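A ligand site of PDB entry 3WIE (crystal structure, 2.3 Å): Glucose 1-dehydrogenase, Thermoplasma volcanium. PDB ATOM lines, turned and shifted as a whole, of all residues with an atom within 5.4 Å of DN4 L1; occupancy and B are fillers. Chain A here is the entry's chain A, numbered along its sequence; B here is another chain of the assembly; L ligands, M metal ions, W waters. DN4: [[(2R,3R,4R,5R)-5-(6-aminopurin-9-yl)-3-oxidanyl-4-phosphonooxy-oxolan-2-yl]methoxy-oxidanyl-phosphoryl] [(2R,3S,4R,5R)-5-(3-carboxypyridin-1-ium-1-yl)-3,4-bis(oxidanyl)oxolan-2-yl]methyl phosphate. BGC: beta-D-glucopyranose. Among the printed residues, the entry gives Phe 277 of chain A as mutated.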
ATOM      1  N   CYS A  41      10.546 -18.473 -19.062  1.00  0.00           N
ATOM      2  CA  CYS A  41       9.820 -19.736 -18.899  1.00  0.00           C
ATOM      3  C   CYS A  41      10.529 -20.446 -17.755  1.00  0.00           C
ATOM      4  O   CYS A  41      11.575 -19.987 -17.270  1.00  0.00           O
ATOM      5  CB  CYS A  41       9.830 -20.592 -20.204  1.00  0.00           C
ATOM      6  SG  CYS A  41      11.382 -21.524 -20.433  1.00  0.00           S
ATOM      7  N   GLY A  42       9.972 -21.541 -17.306  1.00  0.00           N
ATOM      8  CA  GLY A  42      10.483 -22.223 -16.101  1.00  0.00           C
ATOM      9  C   GLY A  42      11.878 -22.756 -16.219  1.00  0.00           C
ATOM     10  O   GLY A  42      12.557 -22.934 -15.198  1.00  0.00           O
ATOM     11  N   THR A  43      12.311 -23.021 -17.436  1.00  0.00           N
ATOM     12  CA  THR A  43      13.686 -23.373 -17.685  1.00  0.00           C
ATOM     13  C   THR A  43      14.630 -22.204 -17.276  1.00  0.00           C
ATOM     14  O   THR A  43      15.601 -22.401 -16.546  1.00  0.00           O
ATOM     15  CB  THR A  43      13.878 -23.732 -19.201  1.00  0.00           C
ATOM     16  OG1 THR A  43      13.140 -24.930 -19.541  1.00  0.00           O
ATOM     17  CG2 THR A  43      15.335 -23.903 -19.533  1.00  0.00           C
ATOM     18  N   ASN A 160       7.337 -25.572 -29.940  1.00  0.00           N
ATOM     19  CA  ASN A 160       7.348 -26.827 -29.221  1.00  0.00           C
ATOM     20  C   ASN A 160       6.006 -27.577 -29.316  1.00  0.00           C
ATOM     21  O   ASN A 160       5.956 -28.810 -29.436  1.00  0.00           O
ATOM     22  CB  ASN A 160       7.676 -26.590 -27.782  1.00  0.00           C
ATOM     23  CG  ASN A 160       9.086 -26.050 -27.589  1.00  0.00           C
ATOM     24  OD1 ASN A 160      10.023 -26.476 -28.242  1.00  0.00           O
ATOM     25  ND2 ASN A 160       9.254 -25.085 -26.675  1.00  0.00           N
ATOM     26  N   ILE A 192      -3.051 -30.993 -19.081  1.00  0.00           N
ATOM     27  CA  ILE A 192      -2.802 -30.779 -17.693  1.00  0.00           C
ATOM     28  C   ILE A 192      -1.966 -29.488 -17.562  1.00  0.00           C
ATOM     29  O   ILE A 192      -0.903 -29.354 -18.164  1.00  0.00           O
ATOM     30  CB  ILE A 192      -2.060 -31.932 -17.086  1.00  0.00           C
ATOM     31  CG1 ILE A 192      -2.821 -33.253 -17.294  1.00  0.00           C
ATOM     32  CG2 ILE A 192      -1.814 -31.705 -15.623  1.00  0.00           C
ATOM     33  CD1 ILE A 192      -1.845 -34.434 -17.276  1.00  0.00           C
ATOM     34  N   GLY A 193      -2.438 -28.591 -16.704  1.00  0.00           N
ATOM     35  CA  GLY A 193      -1.849 -27.286 -16.478  1.00  0.00           C
ATOM     36  C   GLY A 193      -2.642 -26.152 -17.081  1.00  0.00           C
ATOM     37  O   GLY A 193      -3.465 -26.372 -17.934  1.00  0.00           O
ATOM     38  N   SER A 194      -2.424 -24.933 -16.580  1.00  0.00           N
ATOM     39  CA  SER A 194      -3.079 -23.727 -17.092  1.00  0.00           C
ATOM     40  C   SER A 194      -2.134 -22.554 -17.408  1.00  0.00           C
ATOM     41  O   SER A 194      -2.538 -21.416 -17.490  1.00  0.00           O
ATOM     42  CB  SER A 194      -4.212 -23.287 -16.163  1.00  0.00           C
ATOM     43  OG  SER A 194      -3.869 -23.461 -14.829  1.00  0.00           O
ATOM     44  N   GLY A 195      -0.864 -22.870 -17.558  1.00  0.00           N
ATOM     45  CA  GLY A 195       0.206 -21.934 -17.837  1.00  0.00           C
ATOM     46  C   GLY A 195       0.347 -21.639 -19.300  1.00  0.00           C
ATOM     47  O   GLY A 195      -0.544 -21.906 -20.068  1.00  0.00           O
ATOM     48  N   SER A 196       1.449 -21.036 -19.690  1.00  0.00           N
ATOM     49  CA  SER A 196       1.503 -20.556 -21.058  1.00  0.00           C
ATOM     50  C   SER A 196       1.506 -21.683 -22.119  1.00  0.00           C
ATOM     51  O   SER A 196       0.899 -21.557 -23.177  1.00  0.00           O
ATOM     52  CB  SER A 196       2.735 -19.662 -21.246  1.00  0.00           C
ATOM     53  OG  SER A 196       3.859 -20.311 -20.733  1.00  0.00           O
ATOM     54  N   GLU A 197       2.267 -22.737 -21.882  1.00  0.00           N
ATOM     55  CA  GLU A 197       2.347 -23.828 -22.861  1.00  0.00           C
ATOM     56  C   GLU A 197       0.971 -24.529 -22.968  1.00  0.00           C
ATOM     57  O   GLU A 197       0.507 -24.831 -24.078  1.00  0.00           O
ATOM     58  CB  GLU A 197       3.497 -24.806 -22.558  1.00  0.00           C
ATOM     59  CG  GLU A 197       4.926 -24.237 -22.759  1.00  0.00           C
ATOM     60  CD  GLU A 197       5.389 -24.243 -24.237  1.00  0.00           C
ATOM     61  OE1 GLU A 197       6.577 -24.475 -24.544  1.00  0.00           O
ATOM     62  OE2 GLU A 197       4.539 -24.029 -25.120  1.00  0.00           O
ATOM     63  N   ALA A 198       0.282 -24.634 -21.847  1.00  0.00           N
ATOM     64  CA  ALA A 198      -1.081 -25.206 -21.805  1.00  0.00           C
ATOM     65  C   ALA A 198      -2.043 -24.421 -22.666  1.00  0.00           C
ATOM     66  O   ALA A 198      -2.819 -24.993 -23.508  1.00  0.00           O
ATOM     67  CB  ALA A 198      -1.564 -25.318 -20.387  1.00  0.00           C
ATOM     68  N   VAL A 215      -6.905 -28.225 -17.321  1.00  0.00           N
ATOM     69  CA  VAL A 215      -7.261 -28.627 -16.031  1.00  0.00           C
ATOM     70  C   VAL A 215      -6.107 -28.294 -15.065  1.00  0.00           C
ATOM     71  O   VAL A 215      -4.973 -28.204 -15.471  1.00  0.00           O
ATOM     72  CB  VAL A 215      -7.545 -30.137 -15.979  1.00  0.00           C
ATOM     73  CG1 VAL A 215      -8.747 -30.470 -16.848  1.00  0.00           C
ATOM     74  CG2 VAL A 215      -6.329 -30.946 -16.394  1.00  0.00           C
ATOM     75  N   ASN A 216      -6.445 -28.052 -13.791  1.00  0.00           N
ATOM     76  CA  ASN A 216      -5.459 -27.777 -12.730  1.00  0.00           C
ATOM     77  C   ASN A 216      -6.027 -28.161 -11.392  1.00  0.00           C
ATOM     78  O   ASN A 216      -7.230 -28.430 -11.287  1.00  0.00           O
ATOM     79  CB  ASN A 216      -5.029 -26.307 -12.718  1.00  0.00           C
ATOM     80  CG  ASN A 216      -3.635 -26.132 -12.185  1.00  0.00           C
ATOM     81  OD1 ASN A 216      -3.157 -26.893 -11.301  1.00  0.00           O
ATOM     82  ND2 ASN A 216      -2.941 -25.157 -12.712  1.00  0.00           N
ATOM     83  N   ARG A 217      -5.172 -28.215 -10.365  1.00  0.00           N
ATOM     84  CA  ARG A 217      -5.625 -28.601  -9.006  1.00  0.00           C
ATOM     85  C   ARG A 217      -6.128 -27.399  -8.131  1.00  0.00           C
ATOM     86  O   ARG A 217      -6.102 -27.459  -6.911  1.00  0.00           O
ATOM     87  CB  ARG A 217      -4.530 -29.384  -8.266  1.00  0.00           C
ATOM     88  CG  ARG A 217      -3.303 -28.573  -7.885  1.00  0.00           C
ATOM     89  CD  ARG A 217      -2.074 -29.110  -8.602  1.00  0.00           C
ATOM     90  NE  ARG A 217      -0.778 -28.757  -8.000  1.00  0.00           N
ATOM     91  CZ  ARG A 217      -0.086 -27.621  -8.237  1.00  0.00           C
ATOM     92  NH1 ARG A 217       1.087 -27.431  -7.629  1.00  0.00           N
ATOM     93  NH2 ARG A 217      -0.549 -26.664  -9.059  1.00  0.00           N
ATOM     94  N   HIS A 218      -6.586 -26.328  -8.763  1.00  0.00           N
ATOM     95  CA  HIS A 218      -7.105 -25.176  -8.056  1.00  0.00           C
ATOM     96  C   HIS A 218      -7.919 -24.429  -9.078  1.00  0.00           C
ATOM     97  O   HIS A 218      -7.820 -24.758 -10.275  1.00  0.00           O
ATOM     98  CB  HIS A 218      -5.959 -24.289  -7.517  1.00  0.00           C
ATOM     99  CG  HIS A 218      -4.980 -23.819  -8.556  1.00  0.00           C
ATOM    100  ND1 HIS A 218      -5.322 -22.951  -9.569  1.00  0.00           N
ATOM    101  CD2 HIS A 218      -3.651 -24.066  -8.693  1.00  0.00           C
ATOM    102  CE1 HIS A 218      -4.251 -22.692 -10.308  1.00  0.00           C
ATOM    103  NE2 HIS A 218      -3.221 -23.348  -9.789  1.00  0.00           N
ATOM    104  N   GLU A 220      -9.161 -21.122 -11.399  1.00  0.00           N
ATOM    105  CA  GLU A 220      -8.381 -20.202 -12.191  1.00  0.00           C
ATOM    106  C   GLU A 220      -8.911 -18.774 -12.146  1.00  0.00           C
ATOM    107  O   GLU A 220     -10.128 -18.559 -12.135  1.00  0.00           O
ATOM    108  CB  GLU A 220      -8.276 -20.689 -13.670  1.00  0.00           C
ATOM    109  CG  GLU A 220      -7.009 -21.508 -13.936  1.00  0.00           C
ATOM    110  CD  GLU A 220      -5.721 -20.738 -13.713  1.00  0.00           C
ATOM    111  OE1 GLU A 220      -5.785 -19.488 -13.552  1.00  0.00           O
ATOM    112  OE2 GLU A 220      -4.644 -21.377 -13.685  1.00  0.00           O
ATOM    113  N   TYR A 238      -9.574 -30.303 -11.258  1.00  0.00           N
ATOM    114  CA  TYR A 238      -9.803 -31.727 -11.296  1.00  0.00           C
ATOM    115  C   TYR A 238      -9.988 -32.304  -9.894  1.00  0.00           C
ATOM    116  O   TYR A 238     -10.335 -33.465  -9.746  1.00  0.00           O
ATOM    117  CB  TYR A 238      -8.704 -32.470 -12.106  1.00  0.00           C
ATOM    118  CG  TYR A 238      -7.290 -32.329 -11.593  1.00  0.00           C
ATOM    119  CD1 TYR A 238      -6.894 -32.952 -10.425  1.00  0.00           C
ATOM    120  CD2 TYR A 238      -6.328 -31.637 -12.330  1.00  0.00           C
ATOM    121  CE1 TYR A 238      -5.577 -32.847  -9.963  1.00  0.00           C
ATOM    122  CE2 TYR A 238      -5.027 -31.541 -11.882  1.00  0.00           C
ATOM    123  CZ  TYR A 238      -4.654 -32.142 -10.709  1.00  0.00           C
ATOM    124  OH  TYR A 238      -3.335 -32.039 -10.315  1.00  0.00           O
ATOM    125  N   THR A 252       1.707 -30.703 -19.163  1.00  0.00           N
ATOM    126  CA  THR A 252       2.681 -29.608 -19.002  1.00  0.00           C
ATOM    127  C   THR A 252       3.174 -29.506 -17.560  1.00  0.00           C
ATOM    128  O   THR A 252       4.031 -28.714 -17.268  1.00  0.00           O
ATOM    129  CB  THR A 252       2.100 -28.254 -19.462  1.00  0.00           C
ATOM    130  OG1 THR A 252       1.166 -27.757 -18.529  1.00  0.00           O
ATOM    131  CG2 THR A 252       1.397 -28.378 -20.779  1.00  0.00           C
ATOM    132  N   SER A 253       2.678 -30.375 -16.663  1.00  0.00           N
ATOM    133  CA  SER A 253       3.006 -30.311 -15.233  1.00  0.00           C
ATOM    134  C   SER A 253       4.377 -30.918 -14.898  1.00  0.00           C
ATOM    135  O   SER A 253       5.142 -30.388 -14.095  1.00  0.00           O
ATOM    136  CB  SER A 253       1.930 -31.055 -14.435  1.00  0.00           C
ATOM    137  OG  SER A 253       2.091 -32.497 -14.450  1.00  0.00           O
ATOM    138  N   ASP A 255       4.356 -33.740 -13.456  1.00  0.00           N
ATOM    139  CA  ASP A 255       4.056 -34.436 -12.219  1.00  0.00           C
ATOM    140  C   ASP A 255       3.510 -35.854 -12.432  1.00  0.00           C
ATOM    141  O   ASP A 255       2.458 -36.031 -13.014  1.00  0.00           O
ATOM    142  CB  ASP A 255       3.016 -33.646 -11.368  1.00  0.00           C
ATOM    143  CG  ASP A 255       2.821 -34.277 -10.014  1.00  0.00           C
ATOM    144  OD1 ASP A 255       3.846 -34.619  -9.355  1.00  0.00           O
ATOM    145  OD2 ASP A 255       1.667 -34.473  -9.636  1.00  0.00           O
ATOM    146  N   THR A 258      -0.168 -36.710 -11.217  1.00  0.00           N
ATOM    147  CA  THR A 258      -1.150 -36.097 -12.057  1.00  0.00           C
ATOM    148  C   THR A 258      -1.177 -36.851 -13.420  1.00  0.00           C
ATOM    149  O   THR A 258      -2.264 -37.219 -13.935  1.00  0.00           O
ATOM    150  CB  THR A 258      -0.875 -34.595 -12.157  1.00  0.00           C
ATOM    151  OG1 THR A 258      -0.694 -34.065 -10.829  1.00  0.00           O
ATOM    152  CG2 THR A 258      -1.939 -33.870 -12.783  1.00  0.00           C
ATOM    153  N   PHE A 275       5.462 -33.675 -21.918  1.00  0.00           N
ATOM    154  CA  PHE A 275       6.058 -32.440 -22.343  1.00  0.00           C
ATOM    155  C   PHE A 275       6.723 -31.688 -21.205  1.00  0.00           C
ATOM    156  O   PHE A 275       7.874 -31.376 -21.246  1.00  0.00           O
ATOM    157  CB  PHE A 275       4.991 -31.627 -23.025  1.00  0.00           C
ATOM    158  CG  PHE A 275       5.475 -30.358 -23.548  1.00  0.00           C
ATOM    159  CD1 PHE A 275       6.003 -30.293 -24.793  1.00  0.00           C
ATOM    160  CD2 PHE A 275       5.426 -29.234 -22.779  1.00  0.00           C
ATOM    161  CE1 PHE A 275       6.480 -29.129 -25.274  1.00  0.00           C
ATOM    162  CE2 PHE A 275       5.885 -28.057 -23.256  1.00  0.00           C
ATOM    163  CZ  PHE A 275       6.418 -28.001 -24.501  1.00  0.00           C
ATOM    164  N   GLY A 276       5.975 -31.438 -20.158  1.00  0.00           N
ATOM    165  CA  GLY A 276       6.496 -30.778 -19.003  1.00  0.00           C
ATOM    166  C   GLY A 276       7.486 -31.609 -18.251  1.00  0.00           C
ATOM    167  O   GLY A 276       7.417 -32.802 -18.252  1.00  0.00           O
ATOM    168  N   PHE A 277       8.409 -30.948 -17.582  1.00  0.00           N
ATOM    169  CA  PHE A 277       9.370 -31.643 -16.768  1.00  0.00           C
ATOM    170  C   PHE A 277       9.751 -30.864 -15.522  1.00  0.00           C
ATOM    171  O   PHE A 277       9.875 -29.651 -15.516  1.00  0.00           O
ATOM    172  CB  PHE A 277      10.596 -32.093 -17.564  1.00  0.00           C
ATOM    173  CG  PHE A 277      11.466 -30.984 -18.122  1.00  0.00           C
ATOM    174  CD1 PHE A 277      12.433 -30.374 -17.334  1.00  0.00           C
ATOM    175  CD2 PHE A 277      11.372 -30.622 -19.464  1.00  0.00           C
ATOM    176  CE1 PHE A 277      13.262 -29.391 -17.863  1.00  0.00           C
ATOM    177  CE2 PHE A 277      12.197 -29.642 -20.001  1.00  0.00           C
ATOM    178  CZ  PHE A 277      13.138 -29.023 -19.205  1.00  0.00           C
ATOM    179  N   ASN A 278       9.918 -31.635 -14.476  1.00  0.00           N
ATOM    180  CA  ASN A 278      10.162 -31.150 -13.149  1.00  0.00           C
ATOM    181  C   ASN A 278      10.862 -32.286 -12.419  1.00  0.00           C
ATOM    182  O   ASN A 278      10.220 -33.199 -11.941  1.00  0.00           O
ATOM    183  CB  ASN A 278       8.828 -30.814 -12.477  1.00  0.00           C
ATOM    184  CG  ASN A 278       9.010 -30.223 -11.088  1.00  0.00           C
ATOM    185  OD1 ASN A 278      10.139 -29.916 -10.672  1.00  0.00           O
ATOM    186  ND2 ASN A 278       7.901 -30.055 -10.361  1.00  0.00           N
ATOM    187  N   SER A 304       8.143 -35.505 -25.954  1.00  0.00           N
ATOM    188  CA  SER A 304       8.463 -34.523 -26.966  1.00  0.00           C
ATOM    189  C   SER A 304       9.323 -33.408 -26.441  1.00  0.00           C
ATOM    190  O   SER A 304       9.004 -32.799 -25.455  1.00  0.00           O
ATOM    191  CB  SER A 304       7.204 -33.954 -27.548  1.00  0.00           C
ATOM    192  OG  SER A 304       7.365 -33.642 -28.868  1.00  0.00           O
ATOM    193  N   VAL A 305      10.403 -33.095 -27.110  1.00  0.00           N
ATOM    194  CA  VAL A 305      11.167 -31.916 -26.764  1.00  0.00           C
ATOM    195  C   VAL A 305      11.633 -31.194 -27.998  1.00  0.00           C
ATOM    196  O   VAL A 305      12.029 -31.804 -28.960  1.00  0.00           O
ATOM    197  CB  VAL A 305      12.348 -32.239 -25.874  1.00  0.00           C
ATOM    198  CG1 VAL A 305      13.370 -33.035 -26.626  1.00  0.00           C
ATOM    199  CG2 VAL A 305      12.968 -30.985 -25.346  1.00  0.00           C
ATOM    200  N   ASP A 306      11.551 -29.866 -27.952  1.00  0.00           N
ATOM    201  CA  ASP A 306      12.086 -28.945 -28.956  1.00  0.00           C
ATOM    202  C   ASP A 306      11.315 -28.969 -30.251  1.00  0.00           C
ATOM    203  O   ASP A 306      10.283 -29.552 -30.308  1.00  0.00           O
ATOM    204  CB  ASP A 306      13.574 -29.127 -29.153  1.00  0.00           C
ATOM    205  CG  ASP A 306      14.284 -27.827 -29.286  1.00  0.00           C
ATOM    206  OD1 ASP A 306      13.914 -27.049 -30.141  1.00  0.00           O
ATOM    207  OD2 ASP A 306      15.186 -27.554 -28.513  1.00  0.00           O
ATOM    208  N   LYS A 349       7.274 -14.466  -9.583  1.00  0.00           N
ATOM    209  CA  LYS A 349       6.326 -14.340 -10.659  1.00  0.00           C
ATOM    210  C   LYS A 349       5.438 -13.099 -10.483  1.00  0.00           C
ATOM    211  O   LYS A 349       4.821 -12.925  -9.457  1.00  0.00           O
ATOM    212  CB  LYS A 349       5.456 -15.590 -10.719  1.00  0.00           C
ATOM    213  CG  LYS A 349       6.228 -16.896 -10.873  1.00  0.00           C
ATOM    214  CD  LYS A 349       5.386 -18.098 -10.446  1.00  0.00           C
ATOM    215  CE  LYS A 349       4.146 -18.292 -11.315  1.00  0.00           C
ATOM    216  NZ  LYS A 349       4.464 -19.039 -12.553  1.00  0.00           N
ATOM    217  N   ILE A 354       0.998 -15.262 -17.220  1.00  0.00           N
ATOM    218  CA  ILE A 354       0.882 -16.237 -18.252  1.00  0.00           C
ATOM    219  C   ILE A 354       2.254 -16.216 -18.892  1.00  0.00           C
ATOM    220  O   ILE A 354       3.044 -17.078 -18.619  1.00  0.00           O
ATOM    221  CB  ILE A 354      -0.187 -15.889 -19.261  1.00  0.00           C
ATOM    222  CG1 ILE A 354      -1.557 -15.931 -18.616  1.00  0.00           C
ATOM    223  CG2 ILE A 354      -0.165 -16.859 -20.407  1.00  0.00           C
ATOM    224  CD1 ILE A 354      -2.683 -15.461 -19.514  1.00  0.00           C
ATOM    225  N   LYS A 355       2.538 -15.187 -19.669  1.00  0.00           N
ATOM    226  CA  LYS A 355       3.887 -14.967 -20.198  1.00  0.00           C
ATOM    227  C   LYS A 355       4.474 -13.623 -19.826  1.00  0.00           C
ATOM    228  O   LYS A 355       4.044 -12.621 -20.294  1.00  0.00           O
ATOM    229  CB  LYS A 355       3.856 -15.107 -21.717  1.00  0.00           C
ATOM    230  CG  LYS A 355       5.168 -14.928 -22.443  1.00  0.00           C
ATOM    231  CD  LYS A 355       6.248 -15.833 -21.920  1.00  0.00           C
ATOM    232  CE  LYS A 355       6.046 -17.270 -22.334  1.00  0.00           C
ATOM    233  NZ  LYS A 355       6.992 -18.090 -21.557  1.00  0.00           N
ATOM    234  N   VAL B 295      10.986 -37.413 -21.794  1.00  0.00           N
ATOM    235  CA  VAL B 295      10.749 -36.175 -22.595  1.00  0.00           C
ATOM    236  C   VAL B 295      12.001 -35.755 -23.330  1.00  0.00           C
ATOM    237  O   VAL B 295      11.968 -35.629 -24.543  1.00  0.00           O
ATOM    238  CB  VAL B 295      10.278 -35.012 -21.700  1.00  0.00           C
ATOM    239  CG1 VAL B 295      10.164 -33.737 -22.449  1.00  0.00           C
ATOM    240  CG2 VAL B 295       8.935 -35.341 -21.109  1.00  0.00           C
HETATM  241  PA  DN4 L   1       4.396 -22.937 -16.498  1.00  0.00           P
HETATM  242  O1A DN4 L   1       3.657 -21.714 -16.847  1.00  0.00           O
HETATM  243  O2A DN4 L   1       5.086 -23.132 -15.199  1.00  0.00           O
HETATM  244  O5B DN4 L   1       3.235 -24.067 -16.574  1.00  0.00           O
HETATM  245  C5B DN4 L   1       3.153 -25.207 -15.704  1.00  0.00           C
HETATM  246  C4B DN4 L   1       1.670 -25.494 -15.503  1.00  0.00           C
HETATM  247  O4B DN4 L   1       1.569 -26.733 -14.809  1.00  0.00           O
HETATM  248  C3B DN4 L   1       1.039 -24.411 -14.610  1.00  0.00           C
HETATM  249  O3B DN4 L   1      -0.303 -24.147 -15.006  1.00  0.00           O
HETATM  250  C2B DN4 L   1       1.078 -25.070 -13.275  1.00  0.00           C
HETATM  251  O2B DN4 L   1       0.085 -24.461 -12.427  1.00  0.00           O
HETATM  252  C1B DN4 L   1       0.676 -26.472 -13.717  1.00  0.00           C
HETATM  253  N9A DN4 L   1       0.917 -27.515 -12.738  1.00  0.00           N
HETATM  254  C8A DN4 L   1       1.945 -27.767 -11.916  1.00  0.00           C
HETATM  255  N7A DN4 L   1       1.636 -28.860 -11.200  1.00  0.00           N
HETATM  256  C5A DN4 L   1       0.415 -29.276 -11.593  1.00  0.00           C
HETATM  257  C6A DN4 L   1      -0.315 -30.313 -11.235  1.00  0.00           C
HETATM  258  N6A DN4 L   1       0.174 -31.112 -10.300  1.00  0.00           N
HETATM  259  N1A DN4 L   1      -1.516 -30.527 -11.735  1.00  0.00           N
HETATM  260  C2A DN4 L   1      -1.965 -29.662 -12.738  1.00  0.00           C
HETATM  261  N3A DN4 L   1      -1.195 -28.580 -13.136  1.00  0.00           N
HETATM  262  C4A DN4 L   1      -0.022 -28.425 -12.541  1.00  0.00           C
HETATM  263  O3  DN4 L   1       5.494 -23.201 -17.706  1.00  0.00           O
HETATM  264  PN  DN4 L   1       5.162 -23.508 -19.358  1.00  0.00           P
HETATM  265  O1N DN4 L   1       6.074 -22.664 -20.216  1.00  0.00           O
HETATM  266  O2N DN4 L   1       3.685 -23.418 -19.574  1.00  0.00           O
HETATM  267  O5D DN4 L   1       5.665 -25.068 -19.423  1.00  0.00           O
HETATM  268  C5D DN4 L   1       5.568 -25.963 -18.291  1.00  0.00           C
HETATM  269  C4D DN4 L   1       6.535 -27.104 -18.547  1.00  0.00           C
HETATM  270  O4D DN4 L   1       6.901 -27.231 -19.953  1.00  0.00           O
HETATM  271  C3D DN4 L   1       7.847 -26.908 -17.797  1.00  0.00           C
HETATM  272  O3D DN4 L   1       8.114 -28.097 -17.077  1.00  0.00           O
HETATM  273  C2D DN4 L   1       8.899 -26.744 -18.893  1.00  0.00           C
HETATM  274  O2D DN4 L   1      10.128 -27.364 -18.574  1.00  0.00           O
HETATM  275  C1D DN4 L   1       8.299 -27.583 -19.955  1.00  0.00           C
HETATM  276  N1N DN4 L   1       8.804 -27.305 -21.305  1.00  0.00           N
HETATM  277  C2N DN4 L   1       9.045 -28.402 -22.137  1.00  0.00           C
HETATM  278  C3N DN4 L   1       9.482 -28.230 -23.442  1.00  0.00           C
HETATM  279  C7N DN4 L   1       9.743 -29.317 -24.296  1.00  0.00           C
HETATM  280  O7N DN4 L   1       9.634 -30.538 -23.894  1.00  0.00           O
HETATM  281  C4N DN4 L   1       9.639 -26.914 -23.912  1.00  0.00           C
HETATM  282  C5N DN4 L   1       9.373 -25.810 -23.095  1.00  0.00           C
HETATM  283  C6N DN4 L   1       8.958 -25.992 -21.785  1.00  0.00           C
HETATM  284  P2B DN4 L   1       0.518 -23.422 -11.195  1.00  0.00           P
HETATM  285  O1X DN4 L   1       1.215 -22.263 -11.764  1.00  0.00           O
HETATM  286  O2X DN4 L   1      -0.949 -23.095 -10.590  1.00  0.00           O
HETATM  287  O3X DN4 L   1       1.434 -24.330 -10.171  1.00  0.00           O
HETATM  288  O8N DN4 L   1      10.057 -29.015 -25.486  1.00  0.00           O
HETATM  289  C2  BGC L   2      12.888 -24.951 -25.034  1.00  0.00           C
HETATM  290  C3  BGC L   2      13.445 -26.087 -25.906  1.00  0.00           C
HETATM  291  C4  BGC L   2      14.621 -26.802 -25.183  1.00  0.00           C
HETATM  292  C5  BGC L   2      14.109 -27.247 -23.874  1.00  0.00           C
HETATM  293  C6  BGC L   2      15.204 -27.628 -22.921  1.00  0.00           C
HETATM  294  C1  BGC L   2      12.510 -25.540 -23.761  1.00  0.00           C
HETATM  295  O1  BGC L   2      12.257 -24.530 -22.901  1.00  0.00           O
HETATM  296  O2  BGC L   2      11.787 -24.441 -25.596  1.00  0.00           O
HETATM  297  O3  BGC L   2      13.837 -25.569 -27.131  1.00  0.00           O
HETATM  298  O4  BGC L   2      15.039 -27.941 -25.875  1.00  0.00           O
HETATM  299  O5  BGC L   2      13.667 -26.111 -23.205  1.00  0.00           O
HETATM  300  O6  BGC L   2      14.878 -27.012 -21.667  1.00  0.00           O
HETATM  301 ZN    ZN M   1      10.877 -21.592 -22.548  1.00  0.00          ZN
HETATM  302  O   HOH W   1       1.281 -24.676 -19.501  1.00  0.00           O
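NE2 of His 218 lies within hydrogen-bond range of ND2 of Asn 216.
OG of Ser 194 sits at hydrogen-bond distance from OE2 of Glu 220 (2.5 Å).
The backbone NH (N) of Tyr 238 sits at hydrogen-bond distance from the backbone carbonyl oxygen (O) of Asn 216 (3.0 Å).
The side-chain hydroxyl of Thr 258 sits at hydrogen-bond distance from the side-chain hydroxyl of Tyr 238, at 3.4 Å.
The side-chain carboxylate (OE1) of Glu 197 sits at hydrogen-bond distance from the side-chain amide nitrogen (ND2) of Asn 160, 3.5 Å away.
The backbone NH (N) of Gly 193 sits at hydrogen-bond distance from the backbone carbonyl oxygen (O) of Val 215 (2.8 Å).
OG of Ser 253 sits at hydrogen-bond distance from N of Asp 255 (2.8 Å).
The backbone NH (N) of Thr 43 sits close to the side-chain sulfur (SG) of Cys 41, at 3.5 Å.
Water W1 lies within hydrogen-bond range of N of Ala 198 (2.6 Å), O2N of DN4 L1 (2.7 Å), N of Glu 197 (3.2 Å), OG1 of Thr 252 (3.2 Å) and O of Gly 195 (3.4 Å).
An oxygen (O7N) of DN4 L1 lies close to the backbone carbonyl oxygen of Phe 275 (3.3 Å).
Thr 43 touches DN4 L1 (OG1 to O2D, 3.99 Å).
ND2 of Asn 160 touches C4N of DN4 L1, at 3.3 Å.
CG2 of Ile 192 touches C2A of DN4 L1, at 3.5 Å.
Gly 193 touches DN4 L1 (CA to N3A, 3.6 Å).
O of Thr 252 touches C4D of DN4 L1, at 3.2 Å.
Ser 253 touches DN4 L1 (CB to C5A, 3.7 Å).
OD2 of Asp 255 touches N6A of DN4 L1, 3.7 Å away.
Gly 276 touches DN4 L1 (CA to O3D, 3.7 Å).
Val 305 touches DN4 L1.
Val 295 of chain B touches DN4 L1 (CG1 to O7N, 3.6 Å).
Of the 32 residues printed, 23 come within 4 Å of DN4 L1.
An oxygen (O2X) of DN4 L1 lies within hydrogen-bond range of a ring nitrogen (NE2) of His 218 (2.4 Å).
N of Ser 194 is in hydrogen-bond range of O3B of DN4 L1 (2.8 Å).
A nitrogen (N1A) of DN4 L1 is in hydrogen-bond range of the side-chain hydroxyl (OH) of Tyr 238 (2.8 Å).
N of Glu 197 is in hydrogen-bond range of O2N of DN4 L1, at 2.8 Å.
O of Ser 304 lies close to O7N of DN4 L1 (2.8 Å).
The backbone NH (N) of Phe 277 is in hydrogen-bond range of an oxygen (O3D) of DN4 L1, 2.9 Å away.
An oxygen (O3D) of DN4 L1 lies within hydrogen-bond range of the backbone carbonyl oxygen (O) of Phe 277 (2.8 Å).
The backbone NH of Gly 195 lies within hydrogen-bond range of an oxygen (O3B) of DN4 L1.
N of Asp 306 sits at hydrogen-bond distance from O8N of DN4 L1 (3.0 Å).
The side-chain amide nitrogen of Asn 216 is in hydrogen-bond range of an oxygen (O2B) of DN4 L1 (3.1 Å).
A nitrogen (N6A) of DN4 L1 sits at hydrogen-bond distance from the side-chain hydroxyl (OG1) of Thr 258 (3.1 Å).
O3X of DN4 L1 lies within salt-bridge range of NH2 of Arg 217 (3.3 Å).
N of Ser 196 lies within hydrogen-bond range of O2N of DN4 L1 (3.3 Å).
An oxygen (O1N) of DN4 L1 lies within hydrogen-bond range of the side-chain hydroxyl of Ser 196 (3.3 Å).
The side-chain carboxylate (OD2) of Asp 306 lies within hydrogen-bond range of an oxygen (O4) of BGC L2.
An oxygen (O2) of BGC L2 lies within hydrogen-bond range of the side-chain amide nitrogen (ND2) of Asn 160 (2.8 Å).
OG1 of Thr 43 sits at hydrogen-bond distance from O6 of BGC L2.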
